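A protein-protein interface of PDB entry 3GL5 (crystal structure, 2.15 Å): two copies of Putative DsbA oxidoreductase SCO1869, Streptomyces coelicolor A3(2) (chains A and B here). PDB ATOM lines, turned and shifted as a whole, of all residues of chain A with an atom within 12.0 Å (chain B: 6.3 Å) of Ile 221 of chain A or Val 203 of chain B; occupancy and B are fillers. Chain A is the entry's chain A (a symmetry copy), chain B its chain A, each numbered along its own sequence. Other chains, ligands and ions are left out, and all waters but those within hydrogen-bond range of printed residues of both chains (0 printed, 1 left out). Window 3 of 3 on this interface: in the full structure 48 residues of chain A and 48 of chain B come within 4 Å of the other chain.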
ATOM      1  N   PRO A 217     -15.757 -15.360   1.874  1.00  0.00           N
ATOM      2  CA  PRO A 217     -14.599 -16.129   2.320  1.00  0.00           C
ATOM      3  C   PRO A 217     -14.217 -17.225   1.307  1.00  0.00           C
ATOM      4  O   PRO A 217     -15.033 -17.562   0.434  1.00  0.00           O
ATOM      5  CB  PRO A 217     -15.082 -16.704   3.653  1.00  0.00           C
ATOM      6  CG  PRO A 217     -15.973 -15.622   4.193  1.00  0.00           C
ATOM      7  CD  PRO A 217     -16.711 -15.120   2.981  1.00  0.00           C
ATOM      8  N   LEU A 218     -12.993 -17.751   1.400  1.00  0.00           N
ATOM      9  CA  LEU A 218     -12.527 -18.799   0.484  1.00  0.00           C
ATOM     10  C   LEU A 218     -13.253 -20.130   0.645  1.00  0.00           C
ATOM     11  O   LEU A 218     -13.687 -20.482   1.747  1.00  0.00           O
ATOM     12  CB  LEU A 218     -11.044 -19.068   0.687  1.00  0.00           C
ATOM     13  CG  LEU A 218     -10.006 -18.006   0.305  1.00  0.00           C
ATOM     14  CD1 LEU A 218      -8.645 -18.495   0.689  1.00  0.00           C
ATOM     15  CD2 LEU A 218     -10.078 -17.707  -1.176  1.00  0.00           C
ATOM     16  N   LYS A 219     -13.336 -20.888  -0.445  1.00  0.00           N
ATOM     17  CA  LYS A 219     -13.905 -22.229  -0.407  1.00  0.00           C
ATOM     18  C   LYS A 219     -12.762 -23.204  -0.332  1.00  0.00           C
ATOM     19  O   LYS A 219     -11.941 -23.201  -1.206  1.00  0.00           O
ATOM     20  CB  LYS A 219     -14.720 -22.469  -1.674  1.00  0.00           C
ATOM     21  CG  LYS A 219     -16.100 -21.872  -1.586  1.00  0.00           C
ATOM     22  CD  LYS A 219     -16.436 -20.973  -2.744  1.00  0.00           C
ATOM     23  CE  LYS A 219     -17.291 -19.831  -2.226  1.00  0.00           C
ATOM     24  NZ  LYS A 219     -17.883 -19.044  -3.333  1.00  0.00           N
ATOM     25  N   LEU A 220     -12.704 -24.049   0.695  1.00  0.00           N
ATOM     26  CA  LEU A 220     -11.525 -24.921   0.862  1.00  0.00           C
ATOM     27  C   LEU A 220     -11.703 -26.309   0.201  1.00  0.00           C
ATOM     28  O   LEU A 220     -12.836 -26.733  -0.016  1.00  0.00           O
ATOM     29  CB  LEU A 220     -11.109 -25.004   2.349  1.00  0.00           C
ATOM     30  CG  LEU A 220     -10.561 -23.713   3.003  1.00  0.00           C
ATOM     31  CD1 LEU A 220     -11.129 -23.500   4.400  1.00  0.00           C
ATOM     32  CD2 LEU A 220      -9.021 -23.619   3.036  1.00  0.00           C
ATOM     33  N   ILE A 221     -10.601 -26.975  -0.170  1.00  0.00           N
ATOM     34  CA  ILE A 221     -10.635 -28.399  -0.582  1.00  0.00           C
ATOM     35  C   ILE A 221      -9.577 -29.192   0.198  1.00  0.00           C
ATOM     36  O   ILE A 221      -8.392 -28.810   0.202  1.00  0.00           O
ATOM     37  CB  ILE A 221     -10.429 -28.601  -2.087  1.00  0.00           C
ATOM     38  CG1 ILE A 221     -11.567 -27.965  -2.869  1.00  0.00           C
ATOM     39  CG2 ILE A 221     -10.364 -30.075  -2.446  1.00  0.00           C
ATOM     40  CD1 ILE A 221     -11.071 -27.177  -4.017  1.00  0.00           C
ATOM     41  N   ASP A 222     -10.005 -30.293   0.839  1.00  0.00           N
ATOM     42  CA  ASP A 222      -9.191 -31.018   1.837  1.00  0.00           C
ATOM     43  C   ASP A 222      -9.326 -32.529   1.699  1.00  0.00           C
ATOM     44  O   ASP A 222     -10.442 -33.058   1.707  1.00  0.00           O
ATOM     45  CB  ASP A 222      -9.612 -30.579   3.246  1.00  0.00           C
ATOM     46  CG  ASP A 222      -8.531 -30.810   4.301  1.00  0.00           C
ATOM     47  OD1 ASP A 222      -7.407 -31.268   3.974  1.00  0.00           O
ATOM     48  OD2 ASP A 222      -8.830 -30.529   5.486  1.00  0.00           O
ATOM     49  N   ALA A 226      -3.114 -32.874   2.471  1.00  0.00           N
ATOM     50  CA  ALA A 226      -3.735 -32.666   3.787  1.00  0.00           C
ATOM     51  C   ALA A 226      -2.695 -32.287   4.835  1.00  0.00           C
ATOM     52  O   ALA A 226      -2.918 -31.355   5.625  1.00  0.00           O
ATOM     53  CB  ALA A 226      -4.567 -33.903   4.231  1.00  0.00           C
ATOM     54  N   GLU A 227      -1.556 -32.986   4.814  1.00  0.00           N
ATOM     55  CA  GLU A 227      -0.443 -32.747   5.740  1.00  0.00           C
ATOM     56  C   GLU A 227       0.104 -31.318   5.681  1.00  0.00           C
ATOM     57  O   GLU A 227       0.432 -30.817   4.612  1.00  0.00           O
ATOM     58  CB  GLU A 227       0.683 -33.741   5.479  1.00  0.00           C
ATOM     59  CG  GLU A 227       0.426 -35.127   6.038  1.00  0.00           C
ATOM     60  CD  GLU A 227      -0.172 -36.094   5.028  1.00  0.00           C
ATOM     61  OE1 GLU A 227      -0.877 -35.665   4.073  1.00  0.00           O
ATOM     62  OE2 GLU A 227       0.076 -37.309   5.197  1.00  0.00           O
ATOM     63  N   ALA A 228       0.199 -30.687   6.847  1.00  0.00           N
ATOM     64  CA  ALA A 228       0.558 -29.275   6.963  1.00  0.00           C
ATOM     65  C   ALA A 228       1.431 -29.058   8.195  1.00  0.00           C
ATOM     66  O   ALA A 228       1.535 -29.940   9.043  1.00  0.00           O
ATOM     67  CB  ALA A 228      -0.711 -28.425   7.056  1.00  0.00           C
ATOM     68  N   ALA B  26       1.143 -31.328 -10.422  1.00  0.00           N
ATOM     69  CA  ALA B  26      -0.268 -31.180 -10.802  1.00  0.00           C
ATOM     70  C   ALA B  26      -0.442 -30.089 -11.860  1.00  0.00           C
ATOM     71  O   ALA B  26      -1.267 -30.210 -12.795  1.00  0.00           O
ATOM     72  CB  ALA B  26      -1.101 -30.844  -9.581  1.00  0.00           C
ATOM     73  N   TYR B 193     -10.652 -20.299  -3.952  1.00  0.00           N
ATOM     74  CA  TYR B 193     -10.476 -21.576  -3.290  1.00  0.00           C
ATOM     75  C   TYR B 193      -9.185 -21.634  -2.471  1.00  0.00           C
ATOM     76  O   TYR B 193      -8.114 -21.304  -2.971  1.00  0.00           O
ATOM     77  CB  TYR B 193     -10.483 -22.677  -4.343  1.00  0.00           C
ATOM     78  CG  TYR B 193     -11.874 -23.053  -4.801  1.00  0.00           C
ATOM     79  CD1 TYR B 193     -12.584 -24.059  -4.146  1.00  0.00           C
ATOM     80  CD2 TYR B 193     -12.493 -22.398  -5.873  1.00  0.00           C
ATOM     81  CE1 TYR B 193     -13.868 -24.428  -4.554  1.00  0.00           C
ATOM     82  CE2 TYR B 193     -13.788 -22.760  -6.289  1.00  0.00           C
ATOM     83  CZ  TYR B 193     -14.459 -23.773  -5.615  1.00  0.00           C
ATOM     84  OH  TYR B 193     -15.730 -24.149  -5.985  1.00  0.00           O
ATOM     85  N   GLY B 194      -9.290 -22.067  -1.218  1.00  0.00           N
ATOM     86  CA  GLY B 194      -8.109 -22.306  -0.389  1.00  0.00           C
ATOM     87  C   GLY B 194      -7.769 -23.778  -0.298  1.00  0.00           C
ATOM     88  O   GLY B 194      -8.596 -24.581   0.051  1.00  0.00           O
ATOM     89  N   VAL B 195      -6.541 -24.143  -0.598  1.00  0.00           N
ATOM     90  CA  VAL B 195      -6.108 -25.509  -0.372  1.00  0.00           C
ATOM     91  C   VAL B 195      -4.969 -25.567   0.642  1.00  0.00           C
ATOM     92  O   VAL B 195      -3.966 -24.861   0.522  1.00  0.00           O
ATOM     93  CB  VAL B 195      -5.717 -26.193  -1.698  1.00  0.00           C
ATOM     94  CG1 VAL B 195      -5.096 -27.555  -1.428  1.00  0.00           C
ATOM     95  CG2 VAL B 195      -6.969 -26.308  -2.580  1.00  0.00           C
ATOM     96  N   SER B 196      -5.137 -26.425   1.645  1.00  0.00           N
ATOM     97  CA  SER B 196      -4.203 -26.482   2.736  1.00  0.00           C
ATOM     98  C   SER B 196      -3.493 -27.828   2.828  1.00  0.00           C
ATOM     99  O   SER B 196      -4.099 -28.881   2.635  1.00  0.00           O
ATOM    100  CB  SER B 196      -4.931 -26.171   4.041  1.00  0.00           C
ATOM    101  OG  SER B 196      -4.215 -26.730   5.119  1.00  0.00           O
ATOM    102  N   GLN B 199      -1.266 -31.845  -0.285  1.00  0.00           N
ATOM    103  CA  GLN B 199      -2.262 -32.699  -0.895  1.00  0.00           C
ATOM    104  C   GLN B 199      -1.677 -33.557  -2.067  1.00  0.00           C
ATOM    105  O   GLN B 199      -0.618 -33.205  -2.640  1.00  0.00           O
ATOM    106  CB  GLN B 199      -3.368 -31.774  -1.391  1.00  0.00           C
ATOM    107  CG  GLN B 199      -4.022 -30.942  -0.280  1.00  0.00           C
ATOM    108  CD  GLN B 199      -5.287 -31.609   0.284  1.00  0.00           C
ATOM    109  OE1 GLN B 199      -6.172 -32.009  -0.476  1.00  0.00           O
ATOM    110  NE2 GLN B 199      -5.374 -31.724   1.617  1.00  0.00           N
ATOM    111  N   PRO B 200      -2.350 -34.683  -2.409  1.00  0.00           N
ATOM    112  CA  PRO B 200      -2.046 -35.457  -3.629  1.00  0.00           C
ATOM    113  C   PRO B 200      -2.106 -34.570  -4.861  1.00  0.00           C
ATOM    114  O   PRO B 200      -2.934 -33.658  -4.930  1.00  0.00           O
ATOM    115  CB  PRO B 200      -3.197 -36.496  -3.704  1.00  0.00           C
ATOM    116  CG  PRO B 200      -3.715 -36.640  -2.279  1.00  0.00           C
ATOM    117  CD  PRO B 200      -3.316 -35.371  -1.517  1.00  0.00           C
ATOM    118  N   ALA B 201      -1.265 -34.818  -5.849  1.00  0.00           N
ATOM    119  CA  ALA B 201      -1.335 -33.984  -7.042  1.00  0.00           C
ATOM    120  C   ALA B 201      -2.753 -34.004  -7.605  1.00  0.00           C
ATOM    121  O   ALA B 201      -3.172 -33.028  -8.256  1.00  0.00           O
ATOM    122  CB  ALA B 201      -0.279 -34.398  -8.105  1.00  0.00           C
ATOM    123  N   GLU B 202      -3.471 -35.102  -7.314  1.00  0.00           N
ATOM    124  CA  GLU B 202      -4.894 -35.330  -7.672  1.00  0.00           C
ATOM    125  C   GLU B 202      -5.825 -34.258  -7.188  1.00  0.00           C
ATOM    126  O   GLU B 202      -6.639 -33.746  -7.973  1.00  0.00           O
ATOM    127  CB  GLU B 202      -5.452 -36.671  -7.119  1.00  0.00           C
ATOM    128  CG  GLU B 202      -4.776 -37.892  -7.660  1.00  0.00           C
ATOM    129  CD  GLU B 202      -4.151 -37.624  -9.026  1.00  0.00           C
ATOM    130  OE1 GLU B 202      -4.841 -37.054  -9.910  1.00  0.00           O
ATOM    131  OE2 GLU B 202      -2.958 -37.962  -9.200  1.00  0.00           O
ATOM    132  N   VAL B 203      -5.744 -33.966  -5.894  1.00  0.00           N
ATOM    133  CA  VAL B 203      -6.525 -32.898  -5.319  1.00  0.00           C
ATOM    134  C   VAL B 203      -6.113 -31.577  -5.989  1.00  0.00           C
ATOM    135  O   VAL B 203      -6.984 -30.853  -6.493  1.00  0.00           O
ATOM    136  CB  VAL B 203      -6.394 -32.848  -3.792  1.00  0.00           C
ATOM    137  CG1 VAL B 203      -7.321 -31.808  -3.231  1.00  0.00           C
ATOM    138  CG2 VAL B 203      -6.744 -34.219  -3.197  1.00  0.00           C
ATOM    139  N   PHE B 204      -4.803 -31.302  -6.055  1.00  0.00           N
ATOM    140  CA  PHE B 204      -4.328 -30.063  -6.700  1.00  0.00           C
ATOM    141  C   PHE B 204      -4.899 -29.902  -8.118  1.00  0.00           C
ATOM    142  O   PHE B 204      -5.431 -28.859  -8.480  1.00  0.00           O
ATOM    143  CB  PHE B 204      -2.816 -30.001  -6.729  1.00  0.00           C
ATOM    144  CG  PHE B 204      -2.210 -29.661  -5.421  1.00  0.00           C
ATOM    145  CD1 PHE B 204      -2.696 -28.589  -4.674  1.00  0.00           C
ATOM    146  CD2 PHE B 204      -1.170 -30.409  -4.919  1.00  0.00           C
ATOM    147  CE1 PHE B 204      -2.126 -28.254  -3.449  1.00  0.00           C
ATOM    148  CE2 PHE B 204      -0.596 -30.102  -3.682  1.00  0.00           C
ATOM    149  CZ  PHE B 204      -1.066 -29.014  -2.958  1.00  0.00           C
ATOM    150  N   THR B 205      -4.818 -30.974  -8.901  1.00  0.00           N
ATOM    151  CA  THR B 205      -5.400 -31.004 -10.227  1.00  0.00           C
ATOM    152  C   THR B 205      -6.879 -30.610 -10.196  1.00  0.00           C
ATOM    153  O   THR B 205      -7.300 -29.700 -10.920  1.00  0.00           O
ATOM    154  CB  THR B 205      -5.115 -32.389 -10.881  1.00  0.00           C
ATOM    155  OG1 THR B 205      -3.823 -32.320 -11.497  1.00  0.00           O
ATOM    156  CG2 THR B 205      -6.155 -32.773 -11.931  1.00  0.00           C
ATOM    157  N   GLN B 206      -7.635 -31.305  -9.341  1.00  0.00           N
ATOM    158  CA  GLN B 206      -9.046 -31.023  -9.056  1.00  0.00           C
ATOM    159  C   GLN B 206      -9.296 -29.557  -8.715  1.00  0.00           C
ATOM    160  O   GLN B 206     -10.181 -28.919  -9.303  1.00  0.00           O
ATOM    161  CB  GLN B 206      -9.530 -31.891  -7.891  1.00  0.00           C
ATOM    162  CG  GLN B 206     -10.670 -31.274  -7.089  1.00  0.00           C
ATOM    163  CD  GLN B 206     -11.919 -31.026  -7.929  1.00  0.00           C
ATOM    164  OE1 GLN B 206     -12.147 -31.699  -8.939  1.00  0.00           O
ATOM    165  NE2 GLN B 206     -12.738 -30.062  -7.508  1.00  0.00           N
ATOM    166  N   ALA B 207      -8.508 -29.049  -7.764  1.00  0.00           N
ATOM    167  CA  ALA B 207      -8.587 -27.661  -7.293  1.00  0.00           C
ATOM    168  C   ALA B 207      -8.337 -26.673  -8.445  1.00  0.00           C
ATOM    169  O   ALA B 207      -9.125 -25.761  -8.647  1.00  0.00           O
ATOM    170  CB  ALA B 207      -7.597 -27.403  -6.144  1.00  0.00           C
ATOM    171  N   LEU B 208      -7.268 -26.867  -9.195  1.00  0.00           N
ATOM    172  CA  LEU B 208      -7.031 -26.069 -10.403  1.00  0.00           C
ATOM    173  C   LEU B 208      -8.251 -26.060 -11.333  1.00  0.00           C
ATOM    174  O   LEU B 208      -8.681 -25.007 -11.799  1.00  0.00           O
ATOM    175  CB  LEU B 208      -5.794 -26.579 -11.144  1.00  0.00           C
ATOM    176  CG  LEU B 208      -4.461 -26.288 -10.455  1.00  0.00           C
ATOM    177  CD1 LEU B 208      -3.253 -27.125 -10.957  1.00  0.00           C
ATOM    178  CD2 LEU B 208      -4.167 -24.817 -10.544  1.00  0.00           C
ATOM    179  N   GLN B 210     -11.509 -26.915 -10.889  1.00  0.00           N
ATOM    180  CA  GLN B 210     -12.684 -26.323 -10.295  1.00  0.00           C
ATOM    181  C   GLN B 210     -12.541 -24.813 -10.270  1.00  0.00           C
ATOM    182  O   GLN B 210     -13.445 -24.093 -10.678  1.00  0.00           O
ATOM    183  CB  GLN B 210     -12.849 -26.863  -8.874  1.00  0.00           C
ATOM    184  CG  GLN B 210     -14.265 -26.874  -8.386  1.00  0.00           C
ATOM    185  CD  GLN B 210     -14.370 -27.443  -6.996  1.00  0.00           C
ATOM    186  OE1 GLN B 210     -13.487 -28.172  -6.546  1.00  0.00           O
ATOM    187  NE2 GLN B 210     -15.447 -27.110  -6.305  1.00  0.00           N
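The backbone NH (N) of Gly 194 of chain B is in hydrogen-bond range of the backbone carbonyl oxygen (O) of Lys 219 of chain A (2.9 Å). N of Ile 221 of chain A lies within hydrogen-bond range of O of Gly 194 of chain B, at 3.1 Å. The side-chain amide nitrogen (NE2) of Gln 199 of chain B lies within hydrogen-bond range of the side-chain carboxylate (OD1) of Asp 222 of chain A. The backbone NH (N) of Ala 226 of chain A sits close to the side-chain amide nitrogen (NE2) of Gln 199 of chain B (2.7 Å).
OH of Tyr 193 of chain B is in hydrogen-bond range of NE2 of Gln 210 of chain B (3.0 Å). NE2 of Gln 199 of chain B is in hydrogen-bond range of O of Ser 196 of chain B.
Leu 218 of chain A touches Tyr 193 of chain B (CD2 to N, 3.8 Å). Leu 218 of chain A touches Gly 194 of chain B (CB to N, 3.96 Å). O of Lys 219 of chain A touches CA of Tyr 193 of chain B, 3.0 Å away. Leu 220 of chain A touches Gly 194 of chain B (CA to O, 3.1 Å). Ile 221 of chain A touches Tyr 193 of chain B (CD1 to CD1, 3.5 Å). Ile 221 of chain A touches Val 195 of chain B. OE1 of Gln 199 of chain B touches O of Ile 221 of chain A, at 3.95 Å. Ile 221 of chain A touches Val 203 of chain B (CG2 to CG1, 3.6 Å). CD1 of Ile 221 of chain A touches OE1 of Gln 210 of chain B, 3.6 Å away. CA of Ala 226 of chain A touches O of Ser 196 of chain B, at 3.97 Å.
Of the printed residues of chain B, Lys 219 of chain A touches Tyr 193 and Gly 194. Of the printed residues of chain B, Leu 220 of chain A touches Gly 194 (3.1 Å). Of the printed residues of chain B, Ile 221 of chain A touches Tyr 193 (3.5 Å), Gly 194 (3.1 Å), Val 195 (3.9 Å), Gln 199 (3.95 Å), Val 203 (3.6 Å) and Gln 210 (3.6 Å). Of the printed residues of chain B, Ala 226 of chain A touches Ser 196 (3.97 Å) and Gln 199 (2.7 Å). Glu 227 of chain A touches none of the printed residues of chain B. Tyr 193 of chain B touches just these residues of chain A: Leu 218 (3.8 Å), Lys 219 (3.0 Å) and Ile 221 (3.5 Å). Of chain A, only Ala 226 comes within 4 Å of Ser 196 of chain B. Of chain A, only Ile 221, Asp 222 and Ala 226 come within 4 Å of Gln 199 of chain B. Of the printed residues of chain A, Val 203 of chain B touches Ile 221. No residue of chain A comes within 4 Å of Phe 204 of chain B. No residue of chain A comes within 4 Å of Thr 205 of chain B. No residue of chain A comes within 4 Å of Ala 207 of chain B. Of the printed residues of chain A, Gln 210 of chain B touches Ile 221 (3.6 Å). The nearest printed residue of chain B that does not touch Ile 221 of chain A is Ala 207 of chain B (4.1 Å). The nearest printed residue of chain A that does not touch Val 203 of chain B is Asp 222 of chain A (5.1 Å).
Printed residues of chain B that touch a printed residue of chain A: Tyr 193, Gly 194, Val 195, Ser 196, Gln 199, Val 203 and Gln 210. Hydrophobic or aromatic side chains of chain B within 4 Å of the printed part of chain A: Tyr 193, Val 195 and Val 203. Among the printed residues, 14 pairs touch across the chains. Among the printed residues, no Asp or Glu carboxylate lies within 4 Å of a Lys or Arg side-chain nitrogen of the other chain.
No position is printed for both chains. Of the 14 pairs that touch across the chains among the printed residues, none has its exchanged pair printed and touching as well.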
